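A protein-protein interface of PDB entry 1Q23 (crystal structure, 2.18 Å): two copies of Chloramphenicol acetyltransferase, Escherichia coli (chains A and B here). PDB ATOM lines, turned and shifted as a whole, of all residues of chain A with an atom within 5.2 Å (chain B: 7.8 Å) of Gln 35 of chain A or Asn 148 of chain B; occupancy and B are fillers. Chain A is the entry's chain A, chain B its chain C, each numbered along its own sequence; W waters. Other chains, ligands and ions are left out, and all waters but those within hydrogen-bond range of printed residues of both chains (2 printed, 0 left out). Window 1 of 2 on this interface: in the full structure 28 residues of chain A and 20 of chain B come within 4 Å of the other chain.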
ATOM      1  N   TYR A  33      32.452 -18.589 -20.126  1.00  0.00           N
ATOM      2  CA  TYR A  33      31.175 -19.306 -20.034  1.00  0.00           C
ATOM      3  C   TYR A  33      30.039 -18.291 -20.166  1.00  0.00           C
ATOM      4  O   TYR A  33      30.251 -17.089 -19.840  1.00  0.00           O
ATOM      5  CB  TYR A  33      31.101 -20.182 -18.774  1.00  0.00           C
ATOM      6  CG  TYR A  33      31.267 -19.408 -17.465  1.00  0.00           C
ATOM      7  CD1 TYR A  33      30.191 -18.823 -16.813  1.00  0.00           C
ATOM      8  CD2 TYR A  33      32.522 -19.287 -16.869  1.00  0.00           C
ATOM      9  CE1 TYR A  33      30.384 -18.089 -15.524  1.00  0.00           C
ATOM     10  CE2 TYR A  33      32.730 -18.560 -15.698  1.00  0.00           C
ATOM     11  CZ  TYR A  33      31.687 -17.984 -15.027  1.00  0.00           C
ATOM     12  OH  TYR A  33      31.991 -17.289 -13.865  1.00  0.00           O
ATOM     13  N   ASN A  34      28.865 -18.716 -20.702  1.00  0.00           N
ATOM     14  CA  ASN A  34      27.718 -17.807 -20.976  1.00  0.00           C
ATOM     15  C   ASN A  34      26.532 -18.267 -20.102  1.00  0.00           C
ATOM     16  O   ASN A  34      26.351 -19.432 -19.847  1.00  0.00           O
ATOM     17  CB  ASN A  34      27.271 -17.939 -22.421  1.00  0.00           C
ATOM     18  CG  ASN A  34      28.381 -17.563 -23.473  1.00  0.00           C
ATOM     19  OD1 ASN A  34      29.139 -18.411 -23.888  1.00  0.00           O
ATOM     20  ND2 ASN A  34      28.429 -16.325 -23.914  1.00  0.00           N
ATOM     21  N   GLN A  35      25.678 -17.392 -19.641  1.00  0.00           N
ATOM     22  CA  GLN A  35      24.460 -17.928 -19.077  1.00  0.00           C
ATOM     23  C   GLN A  35      23.349 -16.997 -19.438  1.00  0.00           C
ATOM     24  O   GLN A  35      23.597 -15.807 -19.586  1.00  0.00           O
ATOM     25  CB  GLN A  35      24.548 -18.130 -17.562  1.00  0.00           C
ATOM     26  CG  GLN A  35      25.247 -17.150 -16.784  1.00  0.00           C
ATOM     27  CD  GLN A  35      25.469 -17.643 -15.355  1.00  0.00           C
ATOM     28  OE1 GLN A  35      24.551 -18.159 -14.715  1.00  0.00           O
ATOM     29  NE2 GLN A  35      26.688 -17.495 -14.860  1.00  0.00           N
ATOM     30  N   THR A  36      22.126 -17.528 -19.542  1.00  0.00           N
ATOM     31  CA  THR A  36      20.989 -16.676 -19.880  1.00  0.00           C
ATOM     32  C   THR A  36      19.951 -16.724 -18.824  1.00  0.00           C
ATOM     33  O   THR A  36      19.750 -17.755 -18.225  1.00  0.00           O
ATOM     34  CB  THR A  36      20.317 -17.188 -21.223  1.00  0.00           C
ATOM     35  OG1 THR A  36      21.329 -17.092 -22.244  1.00  0.00           O
ATOM     36  CG2 THR A  36      19.172 -16.151 -21.702  1.00  0.00           C
ATOM     37  N   VAL A  37      19.292 -15.594 -18.582  1.00  0.00           N
ATOM     38  CA  VAL A  37      18.249 -15.638 -17.577  1.00  0.00           C
ATOM     39  C   VAL A  37      17.038 -14.904 -18.222  1.00  0.00           C
ATOM     40  O   VAL A  37      17.190 -13.971 -19.065  1.00  0.00           O
ATOM     41  CB  VAL A  37      18.969 -14.929 -16.309  1.00  0.00           C
ATOM     42  CG1 VAL A  37      19.009 -13.431 -16.281  1.00  0.00           C
ATOM     43  CG2 VAL A  37      19.324 -15.787 -15.082  1.00  0.00           C
ATOM     44  N   LEU A 187      18.266 -12.201 -20.946  1.00  0.00           N
ATOM     45  CA  LEU A 187      19.501 -11.500 -20.635  1.00  0.00           C
ATOM     46  C   LEU A 187      20.679 -12.496 -20.574  1.00  0.00           C
ATOM     47  O   LEU A 187      20.577 -13.429 -19.840  1.00  0.00           O
ATOM     48  CB  LEU A 187      19.384 -10.669 -19.365  1.00  0.00           C
ATOM     49  CG  LEU A 187      20.772  -9.940 -19.281  1.00  0.00           C
ATOM     50  CD1 LEU A 187      20.935  -8.753 -20.315  1.00  0.00           C
ATOM     51  CD2 LEU A 187      21.107  -9.432 -17.977  1.00  0.00           C
ATOM     52  N   ALA A 188      21.730 -12.336 -21.407  1.00  0.00           N
ATOM     53  CA  ALA A 188      22.819 -13.318 -21.406  1.00  0.00           C
ATOM     54  C   ALA A 188      24.038 -12.543 -21.003  1.00  0.00           C
ATOM     55  O   ALA A 188      24.090 -11.345 -21.207  1.00  0.00           O
ATOM     56  CB  ALA A 188      23.004 -13.908 -22.768  1.00  0.00           C
ATOM     57  N   ILE A 189      25.001 -13.212 -20.413  1.00  0.00           N
ATOM     58  CA  ILE A 189      26.178 -12.575 -19.893  1.00  0.00           C
ATOM     59  C   ILE A 189      27.283 -13.638 -20.151  1.00  0.00           C
ATOM     60  O   ILE A 189      27.120 -14.829 -19.780  1.00  0.00           O
ATOM     61  CB  ILE A 189      26.115 -12.151 -18.402  1.00  0.00           C
ATOM     62  CG1 ILE A 189      27.537 -11.979 -17.783  1.00  0.00           C
ATOM     63  CG2 ILE A 189      25.532 -13.175 -17.520  1.00  0.00           C
ATOM     64  CD1 ILE A 189      28.256 -10.912 -18.500  1.00  0.00           C
ATOM     65  N   GLN A 190      28.357 -13.195 -20.814  1.00  0.00           N
ATOM     66  CA  GLN A 190      29.540 -14.038 -21.093  1.00  0.00           C
ATOM     67  C   GLN A 190      30.687 -13.461 -20.261  1.00  0.00           C
ATOM     68  O   GLN A 190      30.884 -12.241 -20.293  1.00  0.00           O
ATOM     69  CB  GLN A 190      29.999 -13.907 -22.534  1.00  0.00           C
ATOM     70  CG  GLN A 190      31.119 -14.942 -22.892  1.00  0.00           C
ATOM     71  CD  GLN A 190      32.521 -14.288 -23.174  1.00  0.00           C
ATOM     72  OE1 GLN A 190      33.242 -14.796 -24.033  1.00  0.00           O
ATOM     73  NE2 GLN A 190      32.872 -13.174 -22.484  1.00  0.00           N
ATOM     74  N   GLY A 198      31.183 -18.455 -10.750  1.00  0.00           N
ATOM     75  CA  GLY A 198      29.733 -18.510 -10.745  1.00  0.00           C
ATOM     76  C   GLY A 198      29.156 -17.575  -9.701  1.00  0.00           C
ATOM     77  O   GLY A 198      28.095 -16.932  -9.938  1.00  0.00           O
ATOM     78  N   VAL A 201      29.057 -13.878 -11.101  1.00  0.00           N
ATOM     79  CA  VAL A 201      28.002 -13.599 -12.016  1.00  0.00           C
ATOM     80  C   VAL A 201      26.622 -13.621 -11.298  1.00  0.00           C
ATOM     81  O   VAL A 201      25.824 -12.728 -11.482  1.00  0.00           O
ATOM     82  CB  VAL A 201      28.026 -14.591 -13.177  1.00  0.00           C
ATOM     83  CG1 VAL A 201      27.034 -14.141 -14.231  1.00  0.00           C
ATOM     84  CG2 VAL A 201      29.411 -14.636 -13.790  1.00  0.00           C
ATOM     85  N   GLY A 202      26.393 -14.646 -10.494  1.00  0.00           N
ATOM     86  CA  GLY A 202      25.210 -14.896  -9.649  1.00  0.00           C
ATOM     87  C   GLY A 202      24.916 -13.722  -8.720  1.00  0.00           C
ATOM     88  O   GLY A 202      23.780 -13.232  -8.677  1.00  0.00           O
ATOM     89  N   LEU A 205      23.833 -10.896 -11.048  1.00  0.00           N
ATOM     90  CA  LEU A 205      22.510 -11.071 -11.605  1.00  0.00           C
ATOM     91  C   LEU A 205      21.369 -10.865 -10.554  1.00  0.00           C
ATOM     92  O   LEU A 205      20.274 -10.294 -10.873  1.00  0.00           O
ATOM     93  CB  LEU A 205      22.441 -12.379 -12.355  1.00  0.00           C
ATOM     94  CG  LEU A 205      23.199 -12.433 -13.657  1.00  0.00           C
ATOM     95  CD1 LEU A 205      23.012 -13.971 -14.066  1.00  0.00           C
ATOM     96  CD2 LEU A 205      22.632 -11.471 -14.738  1.00  0.00           C
ATOM     97  N   TYR B  56      22.348 -32.034  -2.656  1.00  0.00           N
ATOM     98  CA  TYR B  56      23.484 -31.991  -3.512  1.00  0.00           C
ATOM     99  C   TYR B  56      24.163 -33.313  -3.664  1.00  0.00           C
ATOM    100  O   TYR B  56      24.352 -33.767  -4.786  1.00  0.00           O
ATOM    101  CB  TYR B  56      24.416 -30.850  -3.035  1.00  0.00           C
ATOM    102  CG  TYR B  56      25.588 -30.449  -3.962  1.00  0.00           C
ATOM    103  CD1 TYR B  56      25.396 -30.186  -5.368  1.00  0.00           C
ATOM    104  CD2 TYR B  56      26.919 -30.273  -3.391  1.00  0.00           C
ATOM    105  CE1 TYR B  56      26.477 -29.775  -6.169  1.00  0.00           C
ATOM    106  CE2 TYR B  56      27.969 -29.883  -4.153  1.00  0.00           C
ATOM    107  CZ  TYR B  56      27.740 -29.648  -5.561  1.00  0.00           C
ATOM    108  OH  TYR B  56      28.815 -29.266  -6.249  1.00  0.00           O
ATOM    109  N   THR B  93      31.711 -28.995  -6.916  1.00  0.00           N
ATOM    110  CA  THR B  93      32.220 -27.766  -6.403  1.00  0.00           C
ATOM    111  C   THR B  93      31.754 -27.691  -4.954  1.00  0.00           C
ATOM    112  O   THR B  93      30.681 -28.144  -4.610  1.00  0.00           O
ATOM    113  CB  THR B  93      31.749 -26.528  -7.191  1.00  0.00           C
ATOM    114  OG1 THR B  93      30.321 -26.551  -7.242  1.00  0.00           O
ATOM    115  CG2 THR B  93      32.225 -26.635  -8.648  1.00  0.00           C
ATOM    116  N   VAL B 145      30.877 -31.535 -11.850  1.00  0.00           N
ATOM    117  CA  VAL B 145      29.535 -31.156 -11.406  1.00  0.00           C
ATOM    118  C   VAL B 145      29.772 -29.838 -10.702  1.00  0.00           C
ATOM    119  O   VAL B 145      30.750 -29.629  -9.876  1.00  0.00           O
ATOM    120  CB  VAL B 145      28.894 -32.101 -10.400  1.00  0.00           C
ATOM    121  CG1 VAL B 145      27.397 -31.680 -10.180  1.00  0.00           C
ATOM    122  CG2 VAL B 145      28.863 -33.530 -10.952  1.00  0.00           C
ATOM    123  N   SER B 146      28.952 -28.911 -11.051  1.00  0.00           N
ATOM    124  CA  SER B 146      29.142 -27.623 -10.504  1.00  0.00           C
ATOM    125  C   SER B 146      27.805 -27.158 -10.058  1.00  0.00           C
ATOM    126  O   SER B 146      26.778 -27.373 -10.771  1.00  0.00           O
ATOM    127  CB  SER B 146      29.836 -26.721 -11.545  1.00  0.00           C
ATOM    128  OG  SER B 146      29.187 -25.507 -11.601  1.00  0.00           O
ATOM    129  N   ALA B 147      27.764 -26.567  -8.862  1.00  0.00           N
ATOM    130  CA  ALA B 147      26.508 -25.995  -8.385  1.00  0.00           C
ATOM    131  C   ALA B 147      26.450 -24.475  -8.520  1.00  0.00           C
ATOM    132  O   ALA B 147      27.399 -23.788  -8.201  1.00  0.00           O
ATOM    133  CB  ALA B 147      26.219 -26.394  -6.915  1.00  0.00           C
ATOM    134  N   ASN B 148      25.315 -23.964  -8.965  1.00  0.00           N
ATOM    135  CA  ASN B 148      25.094 -22.503  -9.196  1.00  0.00           C
ATOM    136  C   ASN B 148      23.728 -22.180  -8.551  1.00  0.00           C
ATOM    137  O   ASN B 148      22.686 -22.237  -9.243  1.00  0.00           O
ATOM    138  CB  ASN B 148      25.022 -22.278 -10.740  1.00  0.00           C
ATOM    139  CG  ASN B 148      25.074 -20.741 -11.206  1.00  0.00           C
ATOM    140  OD1 ASN B 148      25.147 -19.816 -10.367  1.00  0.00           O
ATOM    141  ND2 ASN B 148      25.012 -20.491 -12.572  1.00  0.00           N
ATOM    142  N   PRO B 149      23.634 -21.916  -7.251  1.00  0.00           N
ATOM    143  CA  PRO B 149      22.279 -21.680  -6.760  1.00  0.00           C
ATOM    144  C   PRO B 149      21.932 -20.247  -6.742  1.00  0.00           C
ATOM    145  O   PRO B 149      20.980 -19.934  -6.141  1.00  0.00           O
ATOM    146  CB  PRO B 149      22.335 -22.233  -5.346  1.00  0.00           C
ATOM    147  CG  PRO B 149      23.845 -21.891  -4.862  1.00  0.00           C
ATOM    148  CD  PRO B 149      24.647 -21.874  -6.158  1.00  0.00           C
ATOM    149  N   TRP B 150      22.674 -19.364  -7.369  1.00  0.00           N
ATOM    150  CA  TRP B 150      22.182 -18.049  -7.480  1.00  0.00           C
ATOM    151  C   TRP B 150      21.283 -17.821  -8.643  1.00  0.00           C
ATOM    152  O   TRP B 150      20.535 -16.907  -8.594  1.00  0.00           O
ATOM    153  CB  TRP B 150      23.330 -17.021  -7.536  1.00  0.00           C
ATOM    154  CG  TRP B 150      24.329 -17.395  -6.458  1.00  0.00           C
ATOM    155  CD1 TRP B 150      24.270 -17.063  -5.109  1.00  0.00           C
ATOM    156  CD2 TRP B 150      25.488 -18.206  -6.621  1.00  0.00           C
ATOM    157  NE1 TRP B 150      25.335 -17.622  -4.444  1.00  0.00           N
ATOM    158  CE2 TRP B 150      26.114 -18.308  -5.349  1.00  0.00           C
ATOM    159  CE3 TRP B 150      26.076 -18.847  -7.726  1.00  0.00           C
ATOM    160  CZ2 TRP B 150      27.286 -19.025  -5.146  1.00  0.00           C
ATOM    161  CZ3 TRP B 150      27.256 -19.584  -7.553  1.00  0.00           C
ATOM    162  CH2 TRP B 150      27.858 -19.667  -6.265  1.00  0.00           C
ATOM    163  N   VAL B 151      21.368 -18.621  -9.693  1.00  0.00           N
ATOM    164  CA  VAL B 151      20.731 -18.239 -10.960  1.00  0.00           C
ATOM    165  C   VAL B 151      19.807 -19.353 -11.551  1.00  0.00           C
ATOM    166  O   VAL B 151      20.194 -20.512 -11.682  1.00  0.00           O
ATOM    167  CB  VAL B 151      21.865 -17.816 -12.017  1.00  0.00           C
ATOM    168  CG1 VAL B 151      21.344 -17.626 -13.436  1.00  0.00           C
ATOM    169  CG2 VAL B 151      22.796 -16.611 -11.483  1.00  0.00           C
ATOM    170  N   SER B 152      18.564 -18.999 -11.844  1.00  0.00           N
ATOM    171  CA  SER B 152      17.719 -19.967 -12.453  1.00  0.00           C
ATOM    172  C   SER B 152      17.892 -19.808 -13.929  1.00  0.00           C
ATOM    173  O   SER B 152      16.983 -19.261 -14.607  1.00  0.00           O
ATOM    174  CB  SER B 152      16.179 -19.777 -12.042  1.00  0.00           C
ATOM    175  OG  SER B 152      16.024 -20.101 -10.658  1.00  0.00           O
ATOM    176  N   PHE B 153      18.987 -20.322 -14.471  1.00  0.00           N
ATOM    177  CA  PHE B 153      19.268 -20.014 -15.851  1.00  0.00           C
ATOM    178  C   PHE B 153      18.455 -20.753 -16.889  1.00  0.00           C
ATOM    179  O   PHE B 153      18.066 -21.967 -16.707  1.00  0.00           O
ATOM    180  CB  PHE B 153      20.758 -20.163 -16.091  1.00  0.00           C
ATOM    181  CG  PHE B 153      21.283 -21.520 -15.775  1.00  0.00           C
ATOM    182  CD1 PHE B 153      21.094 -22.586 -16.652  1.00  0.00           C
ATOM    183  CD2 PHE B 153      21.993 -21.707 -14.624  1.00  0.00           C
ATOM    184  CE1 PHE B 153      21.607 -23.836 -16.372  1.00  0.00           C
ATOM    185  CE2 PHE B 153      22.527 -22.926 -14.292  1.00  0.00           C
ATOM    186  CZ  PHE B 153      22.340 -24.019 -15.153  1.00  0.00           C
ATOM    187  N   THR B 154      18.191 -20.063 -18.000  1.00  0.00           N
ATOM    188  CA  THR B 154      17.721 -20.851 -19.155  1.00  0.00           C
ATOM    189  C   THR B 154      18.838 -21.411 -19.971  1.00  0.00           C
ATOM    190  O   THR B 154      18.579 -22.365 -20.749  1.00  0.00           O
ATOM    191  CB  THR B 154      16.632 -20.144 -20.000  1.00  0.00           C
ATOM    192  OG1 THR B 154      17.074 -18.829 -20.391  1.00  0.00           O
ATOM    193  CG2 THR B 154      15.464 -19.820 -19.118  1.00  0.00           C
ATOM    194  N   SER B 155      20.069 -20.885 -19.816  1.00  0.00           N
ATOM    195  CA  SER B 155      21.221 -21.499 -20.509  1.00  0.00           C
ATOM    196  C   SER B 155      22.467 -21.407 -19.627  1.00  0.00           C
ATOM    197  O   SER B 155      22.647 -20.377 -18.965  1.00  0.00           O
ATOM    198  CB  SER B 155      21.526 -20.728 -21.801  1.00  0.00           C
ATOM    199  OG  SER B 155      22.512 -21.493 -22.476  1.00  0.00           O
ATOM    200  N   PHE B 156      23.277 -22.459 -19.609  1.00  0.00           N
ATOM    201  CA  PHE B 156      24.669 -22.366 -19.075  1.00  0.00           C
ATOM    202  C   PHE B 156      25.530 -22.907 -20.142  1.00  0.00           C
ATOM    203  O   PHE B 156      25.293 -23.995 -20.579  1.00  0.00           O
ATOM    204  CB  PHE B 156      24.945 -23.132 -17.758  1.00  0.00           C
ATOM    205  CG  PHE B 156      26.226 -22.739 -17.138  1.00  0.00           C
ATOM    206  CD1 PHE B 156      26.250 -21.646 -16.222  1.00  0.00           C
ATOM    207  CD2 PHE B 156      27.475 -23.430 -17.492  1.00  0.00           C
ATOM    208  CE1 PHE B 156      27.437 -21.257 -15.651  1.00  0.00           C
ATOM    209  CE2 PHE B 156      28.660 -23.039 -16.895  1.00  0.00           C
ATOM    210  CZ  PHE B 156      28.657 -21.943 -15.985  1.00  0.00           C
ATOM    211  N   ASP B 157      26.508 -22.160 -20.596  1.00  0.00           N
ATOM    212  CA  ASP B 157      27.379 -22.699 -21.645  1.00  0.00           C
ATOM    213  C   ASP B 157      28.889 -22.513 -21.447  1.00  0.00           C
ATOM    214  O   ASP B 157      29.348 -21.418 -21.227  1.00  0.00           O
ATOM    215  CB  ASP B 157      26.974 -22.197 -23.086  1.00  0.00           C
ATOM    216  CG  ASP B 157      25.521 -21.837 -23.204  1.00  0.00           C
ATOM    217  OD1 ASP B 157      24.628 -22.746 -23.450  1.00  0.00           O
ATOM    218  OD2 ASP B 157      25.175 -20.609 -23.091  1.00  0.00           O
ATOM    219  N   LEU B 158      29.648 -23.597 -21.536  1.00  0.00           N
ATOM    220  CA  LEU B 158      31.024 -23.606 -21.196  1.00  0.00           C
ATOM    221  C   LEU B 158      31.697 -23.592 -22.569  1.00  0.00           C
ATOM    222  O   LEU B 158      31.332 -24.451 -23.407  1.00  0.00           O
ATOM    223  CB  LEU B 158      31.283 -24.932 -20.530  1.00  0.00           C
ATOM    224  CG  LEU B 158      32.516 -25.149 -19.710  1.00  0.00           C
ATOM    225  CD1 LEU B 158      33.266 -26.626 -19.858  1.00  0.00           C
ATOM    226  CD2 LEU B 158      33.386 -23.965 -19.576  1.00  0.00           C
ATOM    227  N   THR B 172      26.156 -28.634 -14.936  1.00  0.00           N
ATOM    228  CA  THR B 172      26.147 -27.456 -14.170  1.00  0.00           C
ATOM    229  C   THR B 172      24.659 -27.319 -13.729  1.00  0.00           C
ATOM    230  O   THR B 172      23.763 -27.367 -14.588  1.00  0.00           O
ATOM    231  CB  THR B 172      26.460 -26.264 -15.136  1.00  0.00           C
ATOM    232  OG1 THR B 172      27.839 -26.298 -15.572  1.00  0.00           O
ATOM    233  CG2 THR B 172      26.240 -24.922 -14.301  1.00  0.00           C
ATOM    234  N   MET B 173      24.459 -27.226 -12.407  1.00  0.00           N
ATOM    235  CA  MET B 173      23.146 -27.164 -11.845  1.00  0.00           C
ATOM    236  C   MET B 173      22.799 -25.767 -11.446  1.00  0.00           C
ATOM    237  O   MET B 173      23.592 -25.064 -10.815  1.00  0.00           O
ATOM    238  CB  MET B 173      22.978 -28.035 -10.597  1.00  0.00           C
ATOM    239  CG  MET B 173      23.980 -29.153 -10.422  1.00  0.00           C
ATOM    240  SD  MET B 173      23.554 -30.201  -9.033  1.00  0.00           S
ATOM    241  CE  MET B 173      22.177 -29.289  -8.343  1.00  0.00           C
ATOM    242  N   GLY B 174      21.574 -25.358 -11.809  1.00  0.00           N
ATOM    243  CA  GLY B 174      21.108 -24.001 -11.465  1.00  0.00           C
ATOM    244  C   GLY B 174      20.187 -23.914 -10.278  1.00  0.00           C
ATOM    245  O   GLY B 174      20.019 -24.895  -9.594  1.00  0.00           O
ATOM    246  N   LYS B 175      19.619 -22.746 -10.029  1.00  0.00           N
ATOM    247  CA  LYS B 175      18.700 -22.500  -8.937  1.00  0.00           C
ATOM    248  C   LYS B 175      17.270 -23.020  -9.261  1.00  0.00           C
ATOM    249  O   LYS B 175      16.636 -22.534 -10.157  1.00  0.00           O
ATOM    250  CB  LYS B 175      18.571 -21.023  -8.622  1.00  0.00           C
ATOM    251  CG  LYS B 175      17.693 -20.660  -7.403  1.00  0.00           C
ATOM    252  CD  LYS B 175      17.877 -19.114  -7.348  1.00  0.00           C
ATOM    253  CE  LYS B 175      16.969 -18.497  -6.330  1.00  0.00           C
ATOM    254  NZ  LYS B 175      17.389 -19.141  -5.023  1.00  0.00           N
ATOM    255  N   TYR B 176      16.815 -23.974  -8.488  1.00  0.00           N
ATOM    256  CA  TYR B 176      15.484 -24.490  -8.706  1.00  0.00           C
ATOM    257  C   TYR B 176      14.377 -23.566  -8.279  1.00  0.00           C
ATOM    258  O   TYR B 176      14.601 -22.692  -7.485  1.00  0.00           O
ATOM    259  CB  TYR B 176      15.384 -25.867  -8.111  1.00  0.00           C
ATOM    260  CG  TYR B 176      15.205 -25.985  -6.638  1.00  0.00           C
ATOM    261  CD1 TYR B 176      14.149 -25.297  -5.950  1.00  0.00           C
ATOM    262  CD2 TYR B 176      16.047 -26.856  -5.935  1.00  0.00           C
ATOM    263  CE1 TYR B 176      13.990 -25.468  -4.546  1.00  0.00           C
ATOM    264  CE2 TYR B 176      15.921 -27.013  -4.613  1.00  0.00           C
ATOM    265  CZ  TYR B 176      14.893 -26.319  -3.915  1.00  0.00           C
ATOM    266  OH  TYR B 176      14.855 -26.587  -2.589  1.00  0.00           O
ATOM    267  N   MET B 185      14.419 -27.477 -12.029  1.00  0.00           N
ATOM    268  CA  MET B 185      15.801 -27.112 -11.804  1.00  0.00           C
ATOM    269  C   MET B 185      16.635 -27.021 -13.079  1.00  0.00           C
ATOM    270  O   MET B 185      16.838 -28.029 -13.767  1.00  0.00           O
ATOM    271  CB  MET B 185      16.504 -28.154 -10.918  1.00  0.00           C
ATOM    272  CG  MET B 185      17.915 -27.603 -10.369  1.00  0.00           C
ATOM    273  SD  MET B 185      18.902 -28.796  -9.519  1.00  0.00           S
ATOM    274  CE  MET B 185      19.210 -30.050 -10.803  1.00  0.00           C
ATOM    275  N   PRO B 186      17.203 -25.852 -13.355  1.00  0.00           N
ATOM    276  CA  PRO B 186      17.998 -25.675 -14.569  1.00  0.00           C
ATOM    277  C   PRO B 186      19.119 -26.715 -14.499  1.00  0.00           C
ATOM    278  O   PRO B 186      19.686 -26.919 -13.448  1.00  0.00           O
ATOM    279  CB  PRO B 186      18.549 -24.267 -14.393  1.00  0.00           C
ATOM    280  CG  PRO B 186      17.496 -23.524 -13.511  1.00  0.00           C
ATOM    281  CD  PRO B 186      17.139 -24.613 -12.543  1.00  0.00           C
HETATM  282  O   HOH W   1      26.778 -18.167 -11.962  1.00  0.00           O
HETATM  283  O   HOH W   2      23.863 -18.366 -22.452  1.00  0.00           O
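The side-chain hydroxyl of Tyr 33 of chain A sits at hydrogen-bond distance from the backbone NH of Gly 198 of chain A, 3.4 Å away. The backbone NH (N) of Gln 35 of chain A lies within hydrogen-bond range of the backbone carbonyl oxygen (O) of Ile 189 of chain A (2.9 Å). The backbone NH (N) of Lys 175 of chain B lies within hydrogen-bond range of the backbone carbonyl oxygen (O) of Asn 148 of chain B (3.2 Å). The backbone carbonyl oxygen (O) of Val 151 of chain B lies within hydrogen-bond range of the backbone NH (N) of Lys 175 of chain B. The side-chain hydroxyl (OG) of Ser 155 of chain B is in hydrogen-bond range of the side-chain carboxylate (OD1) of Asp 157 of chain B, at 2.6 Å. The backbone NH of Asn 148 of chain B lies within hydrogen-bond range of the backbone carbonyl oxygen of Met 173 of chain B (2.8 Å).
Water W2 lies within hydrogen-bond range of the side-chain carboxylate of Asp 157 of chain B, the side-chain hydroxyl of Thr 36 of chain A, the side-chain hydroxyl of Ser 155 of chain B and the backbone NH of Gln 35 of chain A. Water W1 lies within hydrogen-bond range of the backbone carbonyl oxygen (O) of Gly 198 of chain A (2.7 Å), the side-chain amide oxygen (OD1) of Asn 148 of chain B (2.8 Å) and the side-chain amide nitrogen (NE2) of Gln 35 of chain A (3.0 Å).
Of the 13 printed residues of chain A, 8 touch a printed residue of chain B. Along chain A the printed residues that touch a printed residue of chain B span positions 33 to 205. Of the 23 printed residues of chain B, 8 touch a printed residue of chain A. Among the printed residues, 17 pairs touch across the chains.
The backbone NH (N) of Thr 154 of chain B sits at hydrogen-bond distance from the backbone carbonyl oxygen (O) of Thr 36 of chain A, at 2.8 Å. The backbone NH (N) of Asn 34 of chain A sits at hydrogen-bond distance from the backbone carbonyl oxygen (O) of Asp 157 of chain B, at 2.8 Å. O of Ser 155 of chain B lies within hydrogen-bond range of N of Thr 36 of chain A (3.0 Å). OE1 of Gln 35 of chain A sits at hydrogen-bond distance from ND2 of Asn 148 of chain B (3.2 Å).
No position is printed for both chains. Of the 17 pairs that touch across the chains among the printed residues, none has its exchanged pair printed and touching as well.
Phe 156 of chain B touches Tyr 33 of chain A. Asp 157 of chain B touches Tyr 33 of chain A (O to CA, 3.0 Å). Asn 34 of chain A touches Ser 155 of chain B. Gln 35 of chain A touches Val 151 of chain B. Ser 155 of chain B touches Gln 35 of chain A. CE1 of Phe 156 of chain B touches NE2 of Gln 35 of chain A, at 3.9 Å. Phe 153 of chain B touches Thr 36 of chain A (CA to O, 3.3 Å). CG1 of Val 151 of chain B touches CG2 of Val 37 of chain A, at 3.2 Å. Trp 150 of chain B touches Gly 198 of chain A (CZ3 to C, 3.5 Å). Trp 150 of chain B touches Gly 202 of chain A.
Gln 35 of chain A touches just these residues of chain B: Asn 148 (3.2 Å), Val 151 (3.5 Å), Ser 155 (3.0 Å) and Phe 156 (3.9 Å). Asn 148 of chain B touches just one residue of chain A: Gln 35. Of the printed residues of chain B, Tyr 33 of chain A touches Phe 156 and Asp 157. Of the printed residues of chain A, Ser 155 of chain B touches Asn 34, Gln 35 and Thr 36. Of the printed residues of chain A, Trp 150 of chain B touches Gly 198 and Gly 202. Printed residues of chain B within 4 Å of Gly 202 of chain A: Trp 150 (3.5 Å) and Val 151 (3.5 Å). Leu 158 of chain B touches none of the printed residues of chain A. The nearest residue of chain A that does not touch Asn 148 of chain B is Gly 198 of chain A (4.1 Å). The nearest printed residue of chain B that does not touch Gly 198 of chain A is Asn 148 of chain B (4.1 Å).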
